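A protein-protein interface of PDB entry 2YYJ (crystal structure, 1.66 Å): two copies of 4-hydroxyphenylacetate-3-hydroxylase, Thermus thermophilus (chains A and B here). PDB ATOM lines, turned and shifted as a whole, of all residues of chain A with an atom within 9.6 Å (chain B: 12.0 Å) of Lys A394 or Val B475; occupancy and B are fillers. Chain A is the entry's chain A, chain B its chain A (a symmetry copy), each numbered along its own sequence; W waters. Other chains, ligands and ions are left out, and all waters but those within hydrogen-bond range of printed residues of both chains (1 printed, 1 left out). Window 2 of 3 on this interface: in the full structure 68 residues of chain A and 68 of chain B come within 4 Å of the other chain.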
ATOM      1  N   ASP A 232     -29.590 -28.690   8.415  1.00  0.00           N
ATOM      2  CA  ASP A 232     -29.617 -28.998   9.841  1.00  0.00           C
ATOM      3  C   ASP A 232     -28.733 -28.104  10.705  1.00  0.00           C
ATOM      4  O   ASP A 232     -28.823 -28.137  11.932  1.00  0.00           O
ATOM      5  CB  ASP A 232     -29.243 -30.466  10.068  1.00  0.00           C
ATOM      6  CG  ASP A 232     -30.160 -31.419   9.328  1.00  0.00           C
ATOM      7  OD1 ASP A 232     -31.365 -31.110   9.210  1.00  0.00           O
ATOM      8  OD2 ASP A 232     -29.683 -32.481   8.873  1.00  0.00           O
ATOM      9  N   SER A 233     -27.880 -27.305  10.077  1.00  0.00           N
ATOM     10  CA  SER A 233     -27.007 -26.416  10.836  1.00  0.00           C
ATOM     11  C   SER A 233     -27.810 -25.307  11.509  1.00  0.00           C
ATOM     12  O   SER A 233     -28.556 -24.589  10.848  1.00  0.00           O
ATOM     13  CB  SER A 233     -25.960 -25.784   9.918  1.00  0.00           C
ATOM     14  OG  SER A 233     -25.288 -24.725  10.581  1.00  0.00           O
ATOM     15  N   PRO A 234     -27.680 -25.161  12.837  1.00  0.00           N
ATOM     16  CA  PRO A 234     -28.434 -24.099  13.510  1.00  0.00           C
ATOM     17  C   PRO A 234     -27.893 -22.716  13.137  1.00  0.00           C
ATOM     18  O   PRO A 234     -28.610 -21.718  13.205  1.00  0.00           O
ATOM     19  CB  PRO A 234     -28.253 -24.428  14.993  1.00  0.00           C
ATOM     20  CG  PRO A 234     -26.926 -25.135  15.026  1.00  0.00           C
ATOM     21  CD  PRO A 234     -27.006 -26.032  13.816  1.00  0.00           C
ATOM     22  N   PHE A 235     -26.623 -22.662  12.745  1.00  0.00           N
ATOM     23  CA  PHE A 235     -26.013 -21.394  12.354  1.00  0.00           C
ATOM     24  C   PHE A 235     -26.545 -20.972  10.986  1.00  0.00           C
ATOM     25  O   PHE A 235     -27.004 -19.846  10.808  1.00  0.00           O
ATOM     26  CB  PHE A 235     -24.488 -21.533  12.281  1.00  0.00           C
ATOM     27  CG  PHE A 235     -23.778 -20.256  11.912  1.00  0.00           C
ATOM     28  CD1 PHE A 235     -23.335 -19.382  12.900  1.00  0.00           C
ATOM     29  CD2 PHE A 235     -23.564 -19.921  10.576  1.00  0.00           C
ATOM     30  CE1 PHE A 235     -22.684 -18.191  12.566  1.00  0.00           C
ATOM     31  CE2 PHE A 235     -22.917 -18.734  10.229  1.00  0.00           C
ATOM     32  CZ  PHE A 235     -22.476 -17.866  11.230  1.00  0.00           C
ATOM     33  N   ASP A 236     -26.482 -21.884  10.024  1.00  0.00           N
ATOM     34  CA  ASP A 236     -26.940 -21.594   8.667  1.00  0.00           C
ATOM     35  C   ASP A 236     -28.457 -21.479   8.533  1.00  0.00           C
ATOM     36  O   ASP A 236     -28.956 -20.655   7.764  1.00  0.00           O
ATOM     37  CB  ASP A 236     -26.438 -22.669   7.696  1.00  0.00           C
ATOM     38  CG  ASP A 236     -24.933 -22.627   7.489  1.00  0.00           C
ATOM     39  OD1 ASP A 236     -24.262 -21.760   8.084  1.00  0.00           O
ATOM     40  OD2 ASP A 236     -24.424 -23.470   6.717  1.00  0.00           O
ATOM     41  N   HIS A 237     -29.191 -22.305   9.275  1.00  0.00           N
ATOM     42  CA  HIS A 237     -30.652 -22.302   9.195  1.00  0.00           C
ATOM     43  C   HIS A 237     -31.261 -22.386  10.585  1.00  0.00           C
ATOM     44  O   HIS A 237     -31.904 -23.376  10.941  1.00  0.00           O
ATOM     45  CB  HIS A 237     -31.103 -23.481   8.334  1.00  0.00           C
ATOM     46  CG  HIS A 237     -30.467 -23.496   6.979  1.00  0.00           C
ATOM     47  ND1 HIS A 237     -29.338 -24.232   6.691  1.00  0.00           N
ATOM     48  CD2 HIS A 237     -30.761 -22.804   5.856  1.00  0.00           C
ATOM     49  CE1 HIS A 237     -28.963 -23.991   5.447  1.00  0.00           C
ATOM     50  NE2 HIS A 237     -29.809 -23.127   4.919  1.00  0.00           N
ATOM     51  N   PRO A 238     -31.093 -21.318  11.382  1.00  0.00           N
ATOM     52  CA  PRO A 238     -31.596 -21.227  12.755  1.00  0.00           C
ATOM     53  C   PRO A 238     -33.065 -21.561  12.985  1.00  0.00           C
ATOM     54  O   PRO A 238     -33.420 -22.072  14.050  1.00  0.00           O
ATOM     55  CB  PRO A 238     -31.236 -19.797  13.163  1.00  0.00           C
ATOM     56  CG  PRO A 238     -31.261 -19.054  11.862  1.00  0.00           C
ATOM     57  CD  PRO A 238     -30.580 -20.015  10.923  1.00  0.00           C
ATOM     58  N   SER A 241     -34.428 -25.262  10.256  1.00  0.00           N
ATOM     59  CA  SER A 241     -33.881 -26.553  10.659  1.00  0.00           C
ATOM     60  C   SER A 241     -34.693 -27.158  11.797  1.00  0.00           C
ATOM     61  O   SER A 241     -34.541 -28.341  12.105  1.00  0.00           O
ATOM     62  CB  SER A 241     -32.429 -26.400  11.122  1.00  0.00           C
ATOM     63  OG  SER A 241     -32.357 -25.608  12.297  1.00  0.00           O
ATOM     64  N   PRO A 388     -22.513 -15.954   4.363  1.00  0.00           N
ATOM     65  CA  PRO A 388     -21.578 -17.072   4.230  1.00  0.00           C
ATOM     66  C   PRO A 388     -22.024 -18.136   5.236  1.00  0.00           C
ATOM     67  O   PRO A 388     -22.795 -17.845   6.154  1.00  0.00           O
ATOM     68  CB  PRO A 388     -20.232 -16.442   4.586  1.00  0.00           C
ATOM     69  CG  PRO A 388     -20.612 -15.333   5.521  1.00  0.00           C
ATOM     70  CD  PRO A 388     -21.831 -14.746   4.852  1.00  0.00           C
ATOM     71  N   SER A 389     -21.545 -19.359   5.056  1.00  0.00           N
ATOM     72  CA  SER A 389     -21.903 -20.473   5.928  1.00  0.00           C
ATOM     73  C   SER A 389     -20.928 -20.632   7.086  1.00  0.00           C
ATOM     74  O   SER A 389     -19.851 -20.040   7.086  1.00  0.00           O
ATOM     75  CB  SER A 389     -21.923 -21.767   5.108  1.00  0.00           C
ATOM     76  OG  SER A 389     -21.978 -22.916   5.938  1.00  0.00           O
ATOM     77  N   GLU A 390     -21.315 -21.417   8.085  1.00  0.00           N
ATOM     78  CA  GLU A 390     -20.410 -21.672   9.197  1.00  0.00           C
ATOM     79  C   GLU A 390     -19.191 -22.357   8.574  1.00  0.00           C
ATOM     80  O   GLU A 390     -18.075 -22.253   9.083  1.00  0.00           O
ATOM     81  CB  GLU A 390     -21.061 -22.599  10.229  1.00  0.00           C
ATOM     82  CG  GLU A 390     -21.739 -23.827   9.641  1.00  0.00           C
ATOM     83  CD  GLU A 390     -21.793 -24.985  10.619  1.00  0.00           C
ATOM     84  OE1 GLU A 390     -20.718 -25.537  10.937  1.00  0.00           O
ATOM     85  OE2 GLU A 390     -22.901 -25.346  11.075  1.00  0.00           O
ATOM     86  N   LYS A 391     -19.415 -23.040   7.453  1.00  0.00           N
ATOM     87  CA  LYS A 391     -18.340 -23.740   6.751  1.00  0.00           C
ATOM     88  C   LYS A 391     -17.310 -22.769   6.179  1.00  0.00           C
ATOM     89  O   LYS A 391     -16.133 -23.107   6.051  1.00  0.00           O
ATOM     90  CB  LYS A 391     -18.911 -24.609   5.629  1.00  0.00           C
ATOM     91  CG  LYS A 391     -19.747 -25.781   6.121  1.00  0.00           C
ATOM     92  CD  LYS A 391     -20.206 -26.658   4.966  1.00  0.00           C
ATOM     93  CE  LYS A 391     -20.937 -27.896   5.467  1.00  0.00           C
ATOM     94  NZ  LYS A 391     -21.409 -28.755   4.343  1.00  0.00           N
ATOM     95  N   ASP A 392     -17.752 -21.568   5.820  1.00  0.00           N
ATOM     96  CA  ASP A 392     -16.835 -20.566   5.288  1.00  0.00           C
ATOM     97  C   ASP A 392     -15.973 -20.018   6.421  1.00  0.00           C
ATOM     98  O   ASP A 392     -14.781 -19.767   6.243  1.00  0.00           O
ATOM     99  CB  ASP A 392     -17.614 -19.433   4.618  1.00  0.00           C
ATOM    100  CG  ASP A 392     -18.276 -19.871   3.329  1.00  0.00           C
ATOM    101  OD1 ASP A 392     -17.548 -20.167   2.357  1.00  0.00           O
ATOM    102  OD2 ASP A 392     -19.524 -19.927   3.287  1.00  0.00           O
ATOM    103  N   PHE A 393     -16.574 -19.836   7.593  1.00  0.00           N
ATOM    104  CA  PHE A 393     -15.829 -19.333   8.740  1.00  0.00           C
ATOM    105  C   PHE A 393     -14.818 -20.375   9.202  1.00  0.00           C
ATOM    106  O   PHE A 393     -13.755 -20.035   9.723  1.00  0.00           O
ATOM    107  CB  PHE A 393     -16.781 -18.986   9.888  1.00  0.00           C
ATOM    108  CG  PHE A 393     -17.378 -17.612   9.781  1.00  0.00           C
ATOM    109  CD1 PHE A 393     -16.590 -16.482   9.974  1.00  0.00           C
ATOM    110  CD2 PHE A 393     -18.723 -17.446   9.475  1.00  0.00           C
ATOM    111  CE1 PHE A 393     -17.131 -15.204   9.860  1.00  0.00           C
ATOM    112  CE2 PHE A 393     -19.275 -16.172   9.359  1.00  0.00           C
ATOM    113  CZ  PHE A 393     -18.478 -15.050   9.552  1.00  0.00           C
ATOM    114  N   LYS A 394     -15.156 -21.644   8.998  1.00  0.00           N
ATOM    115  CA  LYS A 394     -14.284 -22.745   9.391  1.00  0.00           C
ATOM    116  C   LYS A 394     -13.242 -23.044   8.317  1.00  0.00           C
ATOM    117  O   LYS A 394     -12.283 -23.779   8.564  1.00  0.00           O
ATOM    118  CB  LYS A 394     -15.115 -24.002   9.664  1.00  0.00           C
ATOM    119  CG  LYS A 394     -16.016 -23.896  10.884  1.00  0.00           C
ATOM    120  CD  LYS A 394     -16.911 -25.120  11.028  1.00  0.00           C
ATOM    121  CE  LYS A 394     -17.730 -25.051  12.307  1.00  0.00           C
ATOM    122  NZ  LYS A 394     -18.605 -26.245  12.481  1.00  0.00           N
ATOM    123  N   GLY A 395     -13.432 -22.464   7.135  1.00  0.00           N
ATOM    124  CA  GLY A 395     -12.515 -22.685   6.031  1.00  0.00           C
ATOM    125  C   GLY A 395     -11.354 -21.707   5.946  1.00  0.00           C
ATOM    126  O   GLY A 395     -11.173 -20.871   6.831  1.00  0.00           O
ATOM    127  N   PRO A 396     -10.553 -21.787   4.871  1.00  0.00           N
ATOM    128  CA  PRO A 396      -9.385 -20.941   4.609  1.00  0.00           C
ATOM    129  C   PRO A 396      -9.609 -19.431   4.659  1.00  0.00           C
ATOM    130  O   PRO A 396      -8.714 -18.683   5.059  1.00  0.00           O
ATOM    131  CB  PRO A 396      -8.934 -21.400   3.226  1.00  0.00           C
ATOM    132  CG  PRO A 396      -9.324 -22.837   3.210  1.00  0.00           C
ATOM    133  CD  PRO A 396     -10.709 -22.792   3.803  1.00  0.00           C
ATOM    134  N   LEU A 397     -10.789 -18.979   4.245  1.00  0.00           N
ATOM    135  CA  LEU A 397     -11.077 -17.549   4.239  1.00  0.00           C
ATOM    136  C   LEU A 397     -11.671 -17.028   5.543  1.00  0.00           C
ATOM    137  O   LEU A 397     -12.004 -15.847   5.649  1.00  0.00           O
ATOM    138  CB  LEU A 397     -12.010 -17.207   3.071  1.00  0.00           C
ATOM    139  CG  LEU A 397     -11.456 -17.559   1.686  1.00  0.00           C
ATOM    140  CD1 LEU A 397     -12.427 -17.098   0.612  1.00  0.00           C
ATOM    141  CD2 LEU A 397     -10.099 -16.902   1.492  1.00  0.00           C
ATOM    142  N   GLY A 398     -11.794 -17.906   6.533  1.00  0.00           N
ATOM    143  CA  GLY A 398     -12.348 -17.502   7.815  1.00  0.00           C
ATOM    144  C   GLY A 398     -11.775 -16.194   8.337  1.00  0.00           C
ATOM    145  O   GLY A 398     -12.529 -15.288   8.695  1.00  0.00           O
ATOM    146  N   PRO A 399     -10.441 -16.061   8.394  1.00  0.00           N
ATOM    147  CA  PRO A 399      -9.798 -14.836   8.882  1.00  0.00           C
ATOM    148  C   PRO A 399     -10.252 -13.572   8.149  1.00  0.00           C
ATOM    149  O   PRO A 399     -10.430 -12.521   8.764  1.00  0.00           O
ATOM    150  CB  PRO A 399      -8.316 -15.128   8.680  1.00  0.00           C
ATOM    151  CG  PRO A 399      -8.245 -16.604   8.923  1.00  0.00           C
ATOM    152  CD  PRO A 399      -9.438 -17.113   8.146  1.00  0.00           C
ATOM    153  N   PHE A 400     -10.426 -13.674   6.835  1.00  0.00           N
ATOM    154  CA  PHE A 400     -10.872 -12.531   6.041  1.00  0.00           C
ATOM    155  C   PHE A 400     -12.309 -12.172   6.402  1.00  0.00           C
ATOM    156  O   PHE A 400     -12.649 -10.999   6.547  1.00  0.00           O
ATOM    157  CB  PHE A 400     -10.792 -12.848   4.545  1.00  0.00           C
ATOM    158  CG  PHE A 400      -9.391 -12.888   4.005  1.00  0.00           C
ATOM    159  CD1 PHE A 400      -8.642 -11.721   3.896  1.00  0.00           C
ATOM    160  CD2 PHE A 400      -8.820 -14.091   3.609  1.00  0.00           C
ATOM    161  CE1 PHE A 400      -7.340 -11.752   3.398  1.00  0.00           C
ATOM    162  CE2 PHE A 400      -7.516 -14.133   3.110  1.00  0.00           C
ATOM    163  CZ  PHE A 400      -6.778 -12.960   3.005  1.00  0.00           C
ATOM    164  N   LEU A 401     -13.155 -13.187   6.549  1.00  0.00           N
ATOM    165  CA  LEU A 401     -14.555 -12.952   6.891  1.00  0.00           C
ATOM    166  C   LEU A 401     -14.691 -12.301   8.260  1.00  0.00           C
ATOM    167  O   LEU A 401     -15.581 -11.480   8.481  1.00  0.00           O
ATOM    168  CB  LEU A 401     -15.337 -14.268   6.855  1.00  0.00           C
ATOM    169  CG  LEU A 401     -15.408 -14.947   5.481  1.00  0.00           C
ATOM    170  CD1 LEU A 401     -16.216 -16.232   5.585  1.00  0.00           C
ATOM    171  CD2 LEU A 401     -16.041 -13.999   4.469  1.00  0.00           C
ATOM    172  N   GLU A 402     -13.809 -12.661   9.186  1.00  0.00           N
ATOM    173  CA  GLU A 402     -13.865 -12.081  10.519  1.00  0.00           C
ATOM    174  C   GLU A 402     -13.556 -10.591  10.465  1.00  0.00           C
ATOM    175  O   GLU A 402     -13.966  -9.828  11.340  1.00  0.00           O
ATOM    176  CB  GLU A 402     -12.888 -12.801  11.455  1.00  0.00           C
ATOM    177  CG  GLU A 402     -13.289 -14.242  11.731  1.00  0.00           C
ATOM    178  CD  GLU A 402     -12.445 -14.895  12.806  1.00  0.00           C
ATOM    179  OE1 GLU A 402     -11.213 -14.985  12.628  1.00  0.00           O
ATOM    180  OE2 GLU A 402     -13.021 -15.321  13.830  1.00  0.00           O
ATOM    181  N   LYS A 413     -18.768 -13.651  13.396  1.00  0.00           N
ATOM    182  CA  LYS A 413     -19.581 -14.859  13.536  1.00  0.00           C
ATOM    183  C   LYS A 413     -20.941 -14.533  14.142  1.00  0.00           C
ATOM    184  O   LYS A 413     -21.966 -15.068  13.713  1.00  0.00           O
ATOM    185  CB  LYS A 413     -18.857 -15.897  14.396  1.00  0.00           C
ATOM    186  CG  LYS A 413     -17.641 -16.518  13.720  1.00  0.00           C
ATOM    187  CD  LYS A 413     -16.934 -17.479  14.663  1.00  0.00           C
ATOM    188  CE  LYS A 413     -15.706 -18.094  14.019  1.00  0.00           C
ATOM    189  NZ  LYS A 413     -14.996 -19.006  14.962  1.00  0.00           N
ATOM    190  N   ALA A 417     -24.509 -14.821  12.264  1.00  0.00           N
ATOM    191  CA  ALA A 417     -25.508 -15.668  12.908  1.00  0.00           C
ATOM    192  C   ALA A 417     -26.827 -14.896  12.976  1.00  0.00           C
ATOM    193  O   ALA A 417     -27.899 -15.446  12.727  1.00  0.00           O
ATOM    194  CB  ALA A 417     -25.053 -16.047  14.313  1.00  0.00           C
ATOM    195  N   ARG B 466     -30.528 -13.033  21.506  1.00  0.00           N
ATOM    196  CA  ARG B 466     -29.154 -13.439  21.791  1.00  0.00           C
ATOM    197  C   ARG B 466     -29.164 -14.864  22.336  1.00  0.00           C
ATOM    198  O   ARG B 466     -28.303 -15.679  21.993  1.00  0.00           O
ATOM    199  CB  ARG B 466     -28.498 -12.505  22.816  1.00  0.00           C
ATOM    200  CG  ARG B 466     -28.269 -11.087  22.324  1.00  0.00           C
ATOM    201  CD  ARG B 466     -27.553 -10.264  23.388  1.00  0.00           C
ATOM    202  NE  ARG B 466     -27.491  -8.848  23.042  1.00  0.00           N
ATOM    203  CZ  ARG B 466     -28.060  -7.883  23.757  1.00  0.00           C
ATOM    204  NH1 ARG B 466     -28.734  -8.181  24.857  1.00  0.00           N
ATOM    205  NH2 ARG B 466     -27.955  -6.620  23.370  1.00  0.00           N
ATOM    206  N   ALA B 467     -30.143 -15.165  23.184  1.00  0.00           N
ATOM    207  CA  ALA B 467     -30.251 -16.500  23.762  1.00  0.00           C
ATOM    208  C   ALA B 467     -30.540 -17.523  22.669  1.00  0.00           C
ATOM    209  O   ALA B 467     -29.973 -18.614  22.660  1.00  0.00           O
ATOM    210  CB  ALA B 467     -31.360 -16.532  24.814  1.00  0.00           C
ATOM    211  N   PHE B 468     -31.417 -17.164  21.738  1.00  0.00           N
ATOM    212  CA  PHE B 468     -31.768 -18.071  20.654  1.00  0.00           C
ATOM    213  C   PHE B 468     -30.557 -18.356  19.773  1.00  0.00           C
ATOM    214  O   PHE B 468     -30.409 -19.455  19.238  1.00  0.00           O
ATOM    215  CB  PHE B 468     -32.888 -17.474  19.795  1.00  0.00           C
ATOM    216  CG  PHE B 468     -33.592 -18.486  18.935  1.00  0.00           C
ATOM    217  CD1 PHE B 468     -34.642 -19.242  19.450  1.00  0.00           C
ATOM    218  CD2 PHE B 468     -33.192 -18.705  17.621  1.00  0.00           C
ATOM    219  CE1 PHE B 468     -35.285 -20.202  18.670  1.00  0.00           C
ATOM    220  CE2 PHE B 468     -33.827 -19.663  16.832  1.00  0.00           C
ATOM    221  CZ  PHE B 468     -34.876 -20.413  17.358  1.00  0.00           C
ATOM    222  N   LEU B 469     -29.689 -17.359  19.631  1.00  0.00           N
ATOM    223  CA  LEU B 469     -28.498 -17.491  18.800  1.00  0.00           C
ATOM    224  C   LEU B 469     -27.356 -18.270  19.448  1.00  0.00           C
ATOM    225  O   LEU B 469     -26.342 -18.525  18.802  1.00  0.00           O
ATOM    226  CB  LEU B 469     -27.999 -16.104  18.382  1.00  0.00           C
ATOM    227  CG  LEU B 469     -28.928 -15.327  17.441  1.00  0.00           C
ATOM    228  CD1 LEU B 469     -28.383 -13.924  17.215  1.00  0.00           C
ATOM    229  CD2 LEU B 469     -29.059 -16.076  16.117  1.00  0.00           C
ATOM    230  N   LYS B 470     -27.504 -18.643  20.717  1.00  0.00           N
ATOM    231  CA  LYS B 470     -26.444 -19.402  21.376  1.00  0.00           C
ATOM    232  C   LYS B 470     -26.196 -20.710  20.631  1.00  0.00           C
ATOM    233  O   LYS B 470     -25.047 -21.119  20.443  1.00  0.00           O
ATOM    234  CB  LYS B 470     -26.805 -19.688  22.837  1.00  0.00           C
ATOM    235  CG  LYS B 470     -26.766 -18.457  23.726  1.00  0.00           C
ATOM    236  CD  LYS B 470     -27.002 -18.820  25.186  1.00  0.00           C
ATOM    237  CE  LYS B 470     -26.932 -17.592  26.079  1.00  0.00           C
ATOM    238  NZ  LYS B 470     -27.128 -17.940  27.514  1.00  0.00           N
ATOM    239  N   GLU B 471     -27.273 -21.356  20.196  1.00  0.00           N
ATOM    240  CA  GLU B 471     -27.158 -22.611  19.462  1.00  0.00           C
ATOM    241  C   GLU B 471     -26.440 -22.412  18.135  1.00  0.00           C
ATOM    242  O   GLU B 471     -25.763 -23.316  17.645  1.00  0.00           O
ATOM    243  CB  GLU B 471     -28.539 -23.218  19.215  1.00  0.00           C
ATOM    244  CG  GLU B 471     -29.076 -24.012  20.393  1.00  0.00           C
ATOM    245  CD  GLU B 471     -28.181 -25.185  20.749  1.00  0.00           C
ATOM    246  OE1 GLU B 471     -27.937 -26.039  19.868  1.00  0.00           O
ATOM    247  OE2 GLU B 471     -27.720 -25.255  21.907  1.00  0.00           O
ATOM    248  N   SER B 472     -26.592 -21.228  17.551  1.00  0.00           N
ATOM    249  CA  SER B 472     -25.937 -20.926  16.286  1.00  0.00           C
ATOM    250  C   SER B 472     -24.426 -20.872  16.470  1.00  0.00           C
ATOM    251  O   SER B 472     -23.679 -21.479  15.705  1.00  0.00           O
ATOM    252  CB  SER B 472     -26.420 -19.583  15.733  1.00  0.00           C
ATOM    253  OG  SER B 472     -27.792 -19.634  15.391  1.00  0.00           O
ATOM    254  N   LEU B 473     -23.979 -20.149  17.493  1.00  0.00           N
ATOM    255  CA  LEU B 473     -22.549 -20.009  17.746  1.00  0.00           C
ATOM    256  C   LEU B 473     -21.890 -21.275  18.284  1.00  0.00           C
ATOM    257  O   LEU B 473     -20.672 -21.423  18.204  1.00  0.00           O
ATOM    258  CB  LEU B 473     -22.285 -18.841  18.705  1.00  0.00           C
ATOM    259  CG  LEU B 473     -22.454 -17.420  18.148  1.00  0.00           C
ATOM    260  CD1 LEU B 473     -21.569 -17.240  16.921  1.00  0.00           C
ATOM    261  CD2 LEU B 473     -23.904 -17.164  17.790  1.00  0.00           C
ATOM    262  N   LYS B 474     -22.686 -22.190  18.823  1.00  0.00           N
ATOM    263  CA  LYS B 474     -22.133 -23.428  19.362  1.00  0.00           C
ATOM    264  C   LYS B 474     -21.493 -24.317  18.298  1.00  0.00           C
ATOM    265  O   LYS B 474     -20.694 -25.193  18.624  1.00  0.00           O
ATOM    266  CB  LYS B 474     -23.215 -24.224  20.094  1.00  0.00           C
ATOM    267  CG  LYS B 474     -23.657 -23.609  21.409  1.00  0.00           C
ATOM    268  CD  LYS B 474     -24.701 -24.477  22.099  1.00  0.00           C
ATOM    269  CE  LYS B 474     -24.154 -25.865  22.411  1.00  0.00           C
ATOM    270  NZ  LYS B 474     -25.164 -26.719  23.098  1.00  0.00           N
ATOM    271  N   VAL B 475     -21.830 -24.097  17.030  1.00  0.00           N
ATOM    272  CA  VAL B 475     -21.269 -24.918  15.962  1.00  0.00           C
ATOM    273  C   VAL B 475     -19.764 -24.727  15.810  1.00  0.00           C
ATOM    274  O   VAL B 475     -19.095 -25.538  15.171  1.00  0.00           O
ATOM    275  CB  VAL B 475     -21.942 -24.629  14.592  1.00  0.00           C
ATOM    276  CG1 VAL B 475     -23.445 -24.824  14.705  1.00  0.00           C
ATOM    277  CG2 VAL B 475     -21.603 -23.218  14.119  1.00  0.00           C
ATOM    278  N   PHE B 476     -19.231 -23.663  16.401  1.00  0.00           N
ATOM    279  CA  PHE B 476     -17.803 -23.391  16.303  1.00  0.00           C
ATOM    280  C   PHE B 476     -17.009 -23.949  17.476  1.00  0.00           C
ATOM    281  O   PHE B 476     -15.778 -23.889  17.479  1.00  0.00           O
ATOM    282  CB  PHE B 476     -17.560 -21.886  16.187  1.00  0.00           C
ATOM    283  CG  PHE B 476     -18.223 -21.261  14.995  1.00  0.00           C
ATOM    284  CD1 PHE B 476     -19.323 -20.423  15.154  1.00  0.00           C
ATOM    285  CD2 PHE B 476     -17.769 -21.535  13.708  1.00  0.00           C
ATOM    286  CE1 PHE B 476     -19.961 -19.869  14.048  1.00  0.00           C
ATOM    287  CE2 PHE B 476     -18.400 -20.986  12.597  1.00  0.00           C
ATOM    288  CZ  PHE B 476     -19.499 -20.151  12.767  1.00  0.00           C
ATOM    289  N   GLU B 477     -17.707 -24.497  18.465  1.00  0.00           N
ATOM    290  CA  GLU B 477     -17.043 -25.064  19.636  1.00  0.00           C
ATOM    291  C   GLU B 477     -16.373 -26.390  19.288  1.00  0.00           C
ATOM    292  O   GLU B 477     -16.712 -27.022  18.287  1.00  0.00           O
ATOM    293  CB  GLU B 477     -18.049 -25.283  20.771  1.00  0.00           C
ATOM    294  CG  GLU B 477     -18.811 -24.034  21.178  1.00  0.00           C
ATOM    295  CD  GLU B 477     -19.632 -24.237  22.436  1.00  0.00           C
ATOM    296  OE1 GLU B 477     -20.354 -25.253  22.520  1.00  0.00           O
ATOM    297  OE2 GLU B 477     -19.561 -23.375  23.338  1.00  0.00           O
HETATM  298  O   HOH W   1     -20.438 -28.377  13.658  1.00  0.00           O
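No position is printed for both chains. Of the 16 pairs that touch across the chains among the printed residues, none has its exchanged pair printed and touching as well.
CB of Phe A235 touches O of Ser B472, 3.5 Å away. CE1 of Phe A235 touches CE1 of Phe B476 (3.5 Å). Phe B468 touches Pro A238 (CE2 to O, 3.7 Å). CG1 of Val B475 touches OE2 of Glu A390, 3.7 Å away. Glu A390 touches Phe B476 (O to CE2, 3.7 Å). CE2 of Phe B476 touches CB of Phe A393, 3.7 Å away. CD1 of Leu B473 touches O of Lys A413 (3.9 Å). Phe B476 touches Lys A413. Ala A417 touches Leu B469. Ala A417 touches Leu B473 (CB to CD2, 3.8 Å).
OG of Ser B472 is in hydrogen-bond range of O of Pro A234, at 3.1 Å. O of Val B475 lies within hydrogen-bond range of NZ of Lys A394 (2.8 Å).
Pro A234 touches just these residues of chain B: Glu B471 (3.4 Å), Ser B472 (3.1 Å) and Val B475 (3.5 Å). Phe A235 touches just these residues of chain B: Ser B472 (3.5 Å), Val B475 (3.8 Å) and Phe B476 (3.5 Å). Of chain B, only Val B475 and Phe B476 come within 4 Å of Glu A390. No residue of chain B comes within 4 Å of Asp A392. Of chain B, only Val B475 (2.8 Å) and Phe B476 (3.8 Å) come within 4 Å of Lys A394. No residue of chain B comes within 4 Å of Gly A395. Pro A396 touches none of the printed residues of chain B. No residue of chain B comes within 4 Å of Gly A398. Phe A400 touches none of the printed residues of chain B. Leu A401 touches none of the printed residues of chain B. Printed residues of chain B within 4 Å of Ala A417: Leu B469 and Leu B473. Of the printed residues of chain A, Leu B469 touches Ala A417. Val B475 touches four residues of chain A. Phe B476 touches just these residues of chain A: Phe A235, Glu A390, Phe A393, Lys A394 and Lys A413. The nearest printed residue of chain A that does not touch Leu B469 is Pro A238 (5.2 Å).
Water W1 bridges the side-chain amino group (NZ) of Lys A394 (3.0 Å) and the backbone carbonyl oxygen (O) of Val B475 (3.5 Å).
Hydrophobic or aromatic side chains of chain A within 4 Å of the printed part of chain B: Pro A234, Phe A235, Phe A393 and Ala A417. Among the printed residues, no Asp or Glu carboxylate lies within 4 Å of a Lys or Arg side-chain nitrogen of the other chain.
The side-chain hydroxyl of Ser A233 sits close to the backbone NH of Phe A235. OG of Ser A233 is in hydrogen-bond range of OE2 of Glu A390 (2.5 Å). The side-chain carboxylate (OD1) of Asp A236 sits at hydrogen-bond distance from the backbone NH (N) of Glu A390 (3.0 Å). The side-chain amino group of Lys A394 is in salt-bridge range of the side-chain carboxylate of Glu A390, at 2.7 Å. OE2 of Glu B471 is in salt-bridge range of NZ of Lys B474 (3.2 Å).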
